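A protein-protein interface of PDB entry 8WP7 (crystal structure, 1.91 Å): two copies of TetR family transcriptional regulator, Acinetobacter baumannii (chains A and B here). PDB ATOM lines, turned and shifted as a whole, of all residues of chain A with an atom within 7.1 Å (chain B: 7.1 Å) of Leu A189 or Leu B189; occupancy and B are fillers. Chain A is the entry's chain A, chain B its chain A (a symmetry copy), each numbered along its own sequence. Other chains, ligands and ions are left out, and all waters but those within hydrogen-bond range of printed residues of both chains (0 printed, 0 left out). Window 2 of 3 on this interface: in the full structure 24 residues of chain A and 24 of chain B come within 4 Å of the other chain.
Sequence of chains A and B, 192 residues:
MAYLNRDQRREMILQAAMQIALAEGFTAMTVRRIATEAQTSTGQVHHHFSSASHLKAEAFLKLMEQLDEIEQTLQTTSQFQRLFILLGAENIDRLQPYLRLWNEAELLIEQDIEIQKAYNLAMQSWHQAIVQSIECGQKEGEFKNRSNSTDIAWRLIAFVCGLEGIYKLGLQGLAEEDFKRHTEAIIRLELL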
ATOM      1  N   ARG A 146      -5.142  12.771   2.179  1.00  0.00           N
ATOM      2  CA  ARG A 146      -5.033  12.899   0.727  1.00  0.00           C
ATOM      3  C   ARG A 146      -4.779  14.345   0.316  1.00  0.00           C
ATOM      4  O   ARG A 146      -3.771  14.659  -0.326  1.00  0.00           O
ATOM      5  CB  ARG A 146      -6.309  12.383   0.061  1.00  0.00           C
ATOM      6  CG  ARG A 146      -6.185  11.022  -0.577  1.00  0.00           C
ATOM      7  CD  ARG A 146      -7.561  10.417  -0.785  1.00  0.00           C
ATOM      8  NE  ARG A 146      -7.614   9.034  -0.334  1.00  0.00           N
ATOM      9  CZ  ARG A 146      -8.554   8.548   0.463  1.00  0.00           C
ATOM     10  NH1 ARG A 146      -9.544   9.307   0.907  1.00  0.00           N
ATOM     11  NH2 ARG A 146      -8.498   7.271   0.829  1.00  0.00           N
ATOM     12  N   SER A 147      -5.701  15.234   0.665  1.00  0.00           N
ATOM     13  CA  SER A 147      -5.591  16.654   0.386  1.00  0.00           C
ATOM     14  C   SER A 147      -5.616  17.421   1.700  1.00  0.00           C
ATOM     15  O   SER A 147      -5.953  16.877   2.757  1.00  0.00           O
ATOM     16  CB  SER A 147      -6.721  17.129  -0.535  1.00  0.00           C
ATOM     17  OG  SER A 147      -7.491  16.032  -1.001  1.00  0.00           O
ATOM     18  N   ARG A 155     -14.666  22.031  -0.493  1.00  0.00           N
ATOM     19  CA  ARG A 155     -15.308  21.109  -1.426  1.00  0.00           C
ATOM     20  C   ARG A 155     -16.549  20.465  -0.814  1.00  0.00           C
ATOM     21  O   ARG A 155     -17.560  20.274  -1.500  1.00  0.00           O
ATOM     22  CB  ARG A 155     -14.305  20.045  -1.869  1.00  0.00           C
ATOM     23  CG  ARG A 155     -13.202  20.594  -2.771  1.00  0.00           C
ATOM     24  CD  ARG A 155     -12.684  19.530  -3.720  1.00  0.00           C
ATOM     25  NE  ARG A 155     -11.844  18.550  -3.043  1.00  0.00           N
ATOM     26  CZ  ARG A 155     -10.520  18.610  -2.971  1.00  0.00           C
ATOM     27  NH1 ARG A 155      -9.842  19.618  -3.498  1.00  0.00           N
ATOM     28  NH2 ARG A 155      -9.857  17.627  -2.363  1.00  0.00           N
ATOM     29  N   THR A 183     -24.011  12.505   0.391  1.00  0.00           N
ATOM     30  CA  THR A 183     -23.036  13.151   1.262  1.00  0.00           C
ATOM     31  C   THR A 183     -22.072  12.130   1.857  1.00  0.00           C
ATOM     32  O   THR A 183     -20.863  12.382   1.940  1.00  0.00           O
ATOM     33  CB  THR A 183     -23.759  13.928   2.362  1.00  0.00           C
ATOM     34  OG1 THR A 183     -24.631  14.893   1.763  1.00  0.00           O
ATOM     35  CG2 THR A 183     -22.763  14.655   3.254  1.00  0.00           C
ATOM     36  N   GLU A 184     -22.583  10.966   2.268  1.00  0.00           N
ATOM     37  CA  GLU A 184     -21.698   9.917   2.767  1.00  0.00           C
ATOM     38  C   GLU A 184     -20.681   9.504   1.715  1.00  0.00           C
ATOM     39  O   GLU A 184     -19.498   9.310   2.022  1.00  0.00           O
ATOM     40  CB  GLU A 184     -22.505   8.698   3.214  1.00  0.00           C
ATOM     41  CG  GLU A 184     -21.625   7.479   3.456  1.00  0.00           C
ATOM     42  CD  GLU A 184     -22.347   6.343   4.146  1.00  0.00           C
ATOM     43  OE1 GLU A 184     -23.519   6.527   4.540  1.00  0.00           O
ATOM     44  OE2 GLU A 184     -21.736   5.262   4.292  1.00  0.00           O
ATOM     45  N   ALA A 185     -21.122   9.356   0.464  1.00  0.00           N
ATOM     46  CA  ALA A 185     -20.211   8.937  -0.591  1.00  0.00           C
ATOM     47  C   ALA A 185     -19.076   9.938  -0.775  1.00  0.00           C
ATOM     48  O   ALA A 185     -17.917   9.544  -0.935  1.00  0.00           O
ATOM     49  CB  ALA A 185     -20.977   8.742  -1.899  1.00  0.00           C
ATOM     50  N   ILE A 186     -19.384  11.238  -0.742  1.00  0.00           N
ATOM     51  CA  ILE A 186     -18.340  12.242  -0.931  1.00  0.00           C
ATOM     52  C   ILE A 186     -17.398  12.279   0.269  1.00  0.00           C
ATOM     53  O   ILE A 186     -16.177  12.369   0.107  1.00  0.00           O
ATOM     54  CB  ILE A 186     -18.962  13.622  -1.217  1.00  0.00           C
ATOM     55  CG1 ILE A 186     -19.791  13.569  -2.503  1.00  0.00           C
ATOM     56  CG2 ILE A 186     -17.882  14.686  -1.333  1.00  0.00           C
ATOM     57  CD1 ILE A 186     -18.964  13.283  -3.741  1.00  0.00           C
ATOM     58  N   ILE A 187     -17.942  12.218   1.489  1.00  0.00           N
ATOM     59  CA  ILE A 187     -17.086  12.169   2.679  1.00  0.00           C
ATOM     60  C   ILE A 187     -16.124  10.988   2.589  1.00  0.00           C
ATOM     61  O   ILE A 187     -14.918  11.127   2.823  1.00  0.00           O
ATOM     62  CB  ILE A 187     -17.937  12.099   3.961  1.00  0.00           C
ATOM     63  CG1 ILE A 187     -18.730  13.391   4.160  1.00  0.00           C
ATOM     64  CG2 ILE A 187     -17.047  11.837   5.172  1.00  0.00           C
ATOM     65  CD1 ILE A 187     -19.782  13.286   5.248  1.00  0.00           C
ATOM     66  N   ARG A 188     -16.646   9.815   2.226  1.00  0.00           N
ATOM     67  CA  ARG A 188     -15.817   8.617   2.135  1.00  0.00           C
ATOM     68  C   ARG A 188     -14.707   8.782   1.105  1.00  0.00           C
ATOM     69  O   ARG A 188     -13.552   8.419   1.357  1.00  0.00           O
ATOM     70  CB  ARG A 188     -16.689   7.409   1.794  1.00  0.00           C
ATOM     71  CG  ARG A 188     -17.487   6.887   2.967  1.00  0.00           C
ATOM     72  CD  ARG A 188     -18.077   5.516   2.678  1.00  0.00           C
ATOM     73  NE  ARG A 188     -18.886   5.056   3.800  1.00  0.00           N
ATOM     74  CZ  ARG A 188     -18.411   4.346   4.814  1.00  0.00           C
ATOM     75  NH1 ARG A 188     -17.143   3.973   4.860  1.00  0.00           N
ATOM     76  NH2 ARG A 188     -19.228   4.005   5.807  1.00  0.00           N
ATOM     77  N   LEU A 189     -15.039   9.315  -0.074  1.00  0.00           N
ATOM     78  CA  LEU A 189     -14.025   9.488  -1.109  1.00  0.00           C
ATOM     79  C   LEU A 189     -12.955  10.478  -0.678  1.00  0.00           C
ATOM     80  O   LEU A 189     -11.770  10.293  -0.977  1.00  0.00           O
ATOM     81  CB  LEU A 189     -14.668   9.950  -2.417  1.00  0.00           C
ATOM     82  CG  LEU A 189     -15.631   8.979  -3.095  1.00  0.00           C
ATOM     83  CD1 LEU A 189     -16.380   9.688  -4.213  1.00  0.00           C
ATOM     84  CD2 LEU A 189     -14.865   7.772  -3.627  1.00  0.00           C
ATOM     85  N   GLU A 190     -13.349  11.542   0.020  1.00  0.00           N
ATOM     86  CA  GLU A 190     -12.379  12.573   0.360  1.00  0.00           C
ATOM     87  C   GLU A 190     -11.502  12.181   1.541  1.00  0.00           C
ATOM     88  O   GLU A 190     -10.319  12.539   1.562  1.00  0.00           O
ATOM     89  CB  GLU A 190     -13.094  13.893   0.651  1.00  0.00           C
ATOM     90  CG  GLU A 190     -13.662  14.554  -0.593  1.00  0.00           C
ATOM     91  CD  GLU A 190     -12.783  15.676  -1.110  1.00  0.00           C
ATOM     92  OE1 GLU A 190     -11.538  15.523  -1.097  1.00  0.00           O
ATOM     93  OE2 GLU A 190     -13.338  16.707  -1.544  1.00  0.00           O
ATOM     94  N   LEU A 191     -12.043  11.445   2.517  1.00  0.00           N
ATOM     95  CA  LEU A 191     -11.363  11.274   3.798  1.00  0.00           C
ATOM     96  C   LEU A 191     -11.162   9.835   4.251  1.00  0.00           C
ATOM     97  O   LEU A 191     -10.371   9.616   5.177  1.00  0.00           O
ATOM     98  CB  LEU A 191     -12.116  12.030   4.905  1.00  0.00           C
ATOM     99  CG  LEU A 191     -12.139  13.550   4.752  1.00  0.00           C
ATOM    100  CD1 LEU A 191     -13.385  14.135   5.397  1.00  0.00           C
ATOM    101  CD2 LEU A 191     -10.875  14.160   5.354  1.00  0.00           C
ATOM    102  N   LEU A 192     -11.836   8.860   3.651  1.00  0.00           N
ATOM    103  CA  LEU A 192     -11.672   7.459   4.047  1.00  0.00           C
ATOM    104  C   LEU A 192     -11.128   6.601   2.908  1.00  0.00           C
ATOM    105  O   LEU A 192     -10.999   5.383   3.046  1.00  0.00           O
ATOM    106  CB  LEU A 192     -12.999   6.875   4.537  1.00  0.00           C
ATOM    107  CG  LEU A 192     -13.666   7.551   5.732  1.00  0.00           C
ATOM    108  CD1 LEU A 192     -14.980   6.861   6.062  1.00  0.00           C
ATOM    109  CD2 LEU A 192     -12.732   7.511   6.926  1.00  0.00           C
ATOM    110  OXT LEU A 192     -10.810   7.096   1.827  1.00  0.00           O
ATOM    111  N   ARG B 146     -17.086   2.418  -9.560  1.00  0.00           N
ATOM    112  CA  ARG B 146     -17.358   2.497  -8.125  1.00  0.00           C
ATOM    113  C   ARG B 146     -18.850   2.636  -7.850  1.00  0.00           C
ATOM    114  O   ARG B 146     -19.454   1.804  -7.164  1.00  0.00           O
ATOM    115  CB  ARG B 146     -16.602   3.680  -7.517  1.00  0.00           C
ATOM    116  CG  ARG B 146     -15.371   3.307  -6.730  1.00  0.00           C
ATOM    117  CD  ARG B 146     -14.468   4.517  -6.574  1.00  0.00           C
ATOM    118  NE  ARG B 146     -13.081   4.195  -6.878  1.00  0.00           N
ATOM    119  CZ  ARG B 146     -12.315   4.904  -7.694  1.00  0.00           C
ATOM    120  NH1 ARG B 146     -12.770   5.992  -8.297  1.00  0.00           N
ATOM    121  NH2 ARG B 146     -11.065   4.510  -7.916  1.00  0.00           N
ATOM    122  N   SER B 147     -19.455   3.699  -8.368  1.00  0.00           N
ATOM    123  CA  SER B 147     -20.877   3.956  -8.233  1.00  0.00           C
ATOM    124  C   SER B 147     -21.502   4.021  -9.619  1.00  0.00           C
ATOM    125  O   SER B 147     -20.807   4.106 -10.636  1.00  0.00           O
ATOM    126  CB  SER B 147     -21.136   5.257  -7.465  1.00  0.00           C
ATOM    127  OG  SER B 147     -19.928   5.792  -6.951  1.00  0.00           O
ATOM    128  N   ARG B 155     -23.928  14.081  -8.689  1.00  0.00           N
ATOM    129  CA  ARG B 155     -22.957  14.584  -7.720  1.00  0.00           C
ATOM    130  C   ARG B 155     -21.982  15.566  -8.361  1.00  0.00           C
ATOM    131  O   ARG B 155     -21.606  16.571  -7.746  1.00  0.00           O
ATOM    132  CB  ARG B 155     -22.211  13.412  -7.084  1.00  0.00           C
ATOM    133  CG  ARG B 155     -23.086  12.571  -6.157  1.00  0.00           C
ATOM    134  CD  ARG B 155     -22.264  11.922  -5.061  1.00  0.00           C
ATOM    135  NE  ARG B 155     -21.466  10.807  -5.558  1.00  0.00           N
ATOM    136  CZ  ARG B 155     -21.842   9.535  -5.525  1.00  0.00           C
ATOM    137  NH1 ARG B 155     -23.025   9.173  -5.054  1.00  0.00           N
ATOM    138  NH2 ARG B 155     -21.004   8.599  -5.968  1.00  0.00           N
ATOM    139  N   THR B 183     -12.367  20.775  -9.329  1.00  0.00           N
ATOM    140  CA  THR B 183     -13.157  19.893 -10.180  1.00  0.00           C
ATOM    141  C   THR B 183     -12.356  18.658 -10.581  1.00  0.00           C
ATOM    142  O   THR B 183     -12.889  17.540 -10.589  1.00  0.00           O
ATOM    143  CB  THR B 183     -13.640  20.656 -11.412  1.00  0.00           C
ATOM    144  OG1 THR B 183     -14.408  21.790 -10.995  1.00  0.00           O
ATOM    145  CG2 THR B 183     -14.511  19.771 -12.291  1.00  0.00           C
ATOM    146  N   GLU B 184     -11.073  18.834 -10.907  1.00  0.00           N
ATOM    147  CA  GLU B 184     -10.234  17.679 -11.216  1.00  0.00           C
ATOM    148  C   GLU B 184     -10.171  16.711 -10.044  1.00  0.00           C
ATOM    149  O   GLU B 184     -10.248  15.490 -10.230  1.00  0.00           O
ATOM    150  CB  GLU B 184      -8.823  18.125 -11.596  1.00  0.00           C
ATOM    151  CG  GLU B 184      -7.840  16.962 -11.633  1.00  0.00           C
ATOM    152  CD  GLU B 184      -6.508  17.319 -12.256  1.00  0.00           C
ATOM    153  OE1 GLU B 184      -6.367  18.452 -12.763  1.00  0.00           O
ATOM    154  OE2 GLU B 184      -5.601  16.459 -12.235  1.00  0.00           O
ATOM    155  N   ALA B 185     -10.025  17.236  -8.827  1.00  0.00           N
ATOM    156  CA  ALA B 185      -9.930  16.370  -7.660  1.00  0.00           C
ATOM    157  C   ALA B 185     -11.190  15.527  -7.490  1.00  0.00           C
ATOM    158  O   ALA B 185     -11.106  14.332  -7.193  1.00  0.00           O
ATOM    159  CB  ALA B 185      -9.663  17.203  -6.407  1.00  0.00           C
ATOM    160  N   ILE B 186     -12.368  16.128  -7.686  1.00  0.00           N
ATOM    161  CA  ILE B 186     -13.609  15.375  -7.519  1.00  0.00           C
ATOM    162  C   ILE B 186     -13.775  14.346  -8.634  1.00  0.00           C
ATOM    163  O   ILE B 186     -14.174  13.205  -8.382  1.00  0.00           O
ATOM    164  CB  ILE B 186     -14.813  16.331  -7.434  1.00  0.00           C
ATOM    165  CG1 ILE B 186     -14.667  17.256  -6.224  1.00  0.00           C
ATOM    166  CG2 ILE B 186     -16.116  15.550  -7.343  1.00  0.00           C
ATOM    167  CD1 ILE B 186     -14.696  16.522  -4.898  1.00  0.00           C
ATOM    168  N   ILE B 187     -13.482  14.728  -9.882  1.00  0.00           N
ATOM    169  CA  ILE B 187     -13.544  13.763 -10.984  1.00  0.00           C
ATOM    170  C   ILE B 187     -12.646  12.565 -10.689  1.00  0.00           C
ATOM    171  O   ILE B 187     -13.055  11.407 -10.836  1.00  0.00           O
ATOM    172  CB  ILE B 187     -13.162  14.432 -12.318  1.00  0.00           C
ATOM    173  CG1 ILE B 187     -14.200  15.480 -12.719  1.00  0.00           C
ATOM    174  CG2 ILE B 187     -13.026  13.381 -13.416  1.00  0.00           C
ATOM    175  CD1 ILE B 187     -13.751  16.357 -13.873  1.00  0.00           C
ATOM    176  N   ARG B 188     -11.415  12.832 -10.249  1.00  0.00           N
ATOM    177  CA  ARG B 188     -10.468  11.759  -9.962  1.00  0.00           C
ATOM    178  C   ARG B 188     -10.984  10.835  -8.867  1.00  0.00           C
ATOM    179  O   ARG B 188     -10.895   9.607  -8.982  1.00  0.00           O
ATOM    180  CB  ARG B 188      -9.117  12.354  -9.568  1.00  0.00           C
ATOM    181  CG  ARG B 188      -8.319  12.877 -10.741  1.00  0.00           C
ATOM    182  CD  ARG B 188      -6.875  13.156 -10.358  1.00  0.00           C
ATOM    183  NE  ARG B 188      -6.139  13.709 -11.488  1.00  0.00           N
ATOM    184  CZ  ARG B 188      -5.485  12.976 -12.378  1.00  0.00           C
ATOM    185  NH1 ARG B 188      -5.431  11.658 -12.278  1.00  0.00           N
ATOM    186  NH2 ARG B 188      -4.874  13.579 -13.393  1.00  0.00           N
ATOM    187  N   LEU B 189     -11.517  11.406  -7.783  1.00  0.00           N
ATOM    188  CA  LEU B 189     -12.017  10.578  -6.692  1.00  0.00           C
ATOM    189  C   LEU B 189     -13.200   9.731  -7.134  1.00  0.00           C
ATOM    190  O   LEU B 189     -13.335   8.574  -6.720  1.00  0.00           O
ATOM    191  CB  LEU B 189     -12.415  11.446  -5.498  1.00  0.00           C
ATOM    192  CG  LEU B 189     -11.298  12.220  -4.803  1.00  0.00           C
ATOM    193  CD1 LEU B 189     -11.893  13.230  -3.832  1.00  0.00           C
ATOM    194  CD2 LEU B 189     -10.364  11.253  -4.083  1.00  0.00           C
ATOM    195  N   GLU B 190     -14.073  10.287  -7.973  1.00  0.00           N
ATOM    196  CA  GLU B 190     -15.278   9.557  -8.338  1.00  0.00           C
ATOM    197  C   GLU B 190     -15.016   8.491  -9.393  1.00  0.00           C
ATOM    198  O   GLU B 190     -15.649   7.431  -9.354  1.00  0.00           O
ATOM    199  CB  GLU B 190     -16.354  10.527  -8.827  1.00  0.00           C
ATOM    200  CG  GLU B 190     -16.958  11.364  -7.711  1.00  0.00           C
ATOM    201  CD  GLU B 190     -18.299  10.833  -7.246  1.00  0.00           C
ATOM    202  OE1 GLU B 190     -18.455   9.593  -7.138  1.00  0.00           O
ATOM    203  OE2 GLU B 190     -19.195  11.658  -6.971  1.00  0.00           O
ATOM    204  N   LEU B 191     -14.091   8.737 -10.327  1.00  0.00           N
ATOM    205  CA  LEU B 191     -13.985   7.904 -11.522  1.00  0.00           C
ATOM    206  C   LEU B 191     -12.607   7.323 -11.801  1.00  0.00           C
ATOM    207  O   LEU B 191     -12.511   6.409 -12.629  1.00  0.00           O
ATOM    208  CB  LEU B 191     -14.439   8.692 -12.762  1.00  0.00           C
ATOM    209  CG  LEU B 191     -15.915   9.087 -12.774  1.00  0.00           C
ATOM    210  CD1 LEU B 191     -16.122  10.361 -13.578  1.00  0.00           C
ATOM    211  CD2 LEU B 191     -16.763   7.945 -13.330  1.00  0.00           C
ATOM    212  N   LEU B 192     -11.549   7.808 -11.159  1.00  0.00           N
ATOM    213  CA  LEU B 192     -10.203   7.279 -11.389  1.00  0.00           C
ATOM    214  C   LEU B 192      -9.602   6.672 -10.124  1.00  0.00           C
ATOM    215  O   LEU B 192      -8.445   6.247 -10.120  1.00  0.00           O
ATOM    216  CB  LEU B 192      -9.273   8.371 -11.922  1.00  0.00           C
ATOM    217  CG  LEU B 192      -9.665   9.048 -13.234  1.00  0.00           C
ATOM    218  CD1 LEU B 192      -8.650  10.119 -13.597  1.00  0.00           C
ATOM    219  CD2 LEU B 192      -9.754   8.009 -14.334  1.00  0.00           C
ATOM    220  OXT LEU B 192     -10.248   6.597  -9.078  1.00  0.00           O
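The guanidinium group (NE) of Arg A155 is in salt-bridge range of the side-chain carboxylate (OE2) of Glu A190 (2.8 Å).
The backbone carbonyl oxygen of Leu B189 is in hydrogen-bond range of the guanidinium group of Arg B146, 3.1 Å away.
The guanidinium group (NH1) of Arg A146 lies within hydrogen-bond range of the backbone carbonyl oxygen (O) of Glu A190 (3.4 Å).
NH1 of Arg B146 sits at hydrogen-bond distance from O of Glu B190 (3.4 Å).
The side-chain hydroxyl (OG) of Ser B147 lies within hydrogen-bond range of the guanidinium group (NH2) of Arg B155 (3.2 Å).
The side-chain carboxylate (OE2) of Glu B190 lies within salt-bridge range of the guanidinium group (NE) of Arg B155, 2.8 Å away.
Arg A155 touches Ala B185, and with the chains exchanged Ala A185 touches Arg B155.
Arg A155 touches Ile B186, and with the chains exchanged Ile A186 touches Arg B155.
Ile A186 touches Glu B190, and with the chains exchanged Glu A190 touches Ile B186.
Leu A189 touches its own counterpart, Leu B189.
Of the 9 pairs that touch across the chains among the printed residues, 9 have their exchanged pair printed and touching as well.
Hydrophobic or aromatic side chains of chain A within 4 Å of the printed part of chain B: Ala A185, Ile A186 and Leu A189.
Of the 13 printed residues of chain B, 5 touch a printed residue of chain A.
Hydrophobic or aromatic side chains of chain B within 4 Å of the printed part of chain A: Ala B185, Ile B186 and Leu B189.
Among the printed residues, no Asp or Glu carboxylate lies within 4 Å of a Lys or Arg side-chain nitrogen of the other chain.
Of chain B, only Leu B189 and Glu B190 come within 4 Å of Leu A189.
Of chain A, only Leu A189 (3.5 Å) and Glu A190 (3.6 Å) come within 4 Å of Leu B189.
Of the printed residues of chain B, Glu A190 touches Ile B186 and Leu B189.
Printed residues of chain B within 4 Å of Arg A155: Ala B185 (3.8 Å) and Ile B186 (3.8 Å).
The nearest residue of chain A that does not touch Leu B189 is Arg A146 (4.4 Å).
Ala B185 touches Arg A155 (CB to NH1, 3.8 Å).
CD1 of Ile B186 touches CD of Arg A155, at 3.8 Å.
NH1 of Arg B155 touches CB of Ala A185 (3.8 Å).
Ile A186 touches Arg B155 (CD1 to CD, 3.8 Å).
Glu B190 touches Ile A186 (OE2 to CD1, 3.6 Å).
O of Leu A189 touches CD2 of Leu B189 (3.5 Å).
OE1 of Glu B190 touches CD1 of Leu A189 (3.6 Å).
Glu A190 touches Ile B186.
Leu B189 touches Glu A190.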
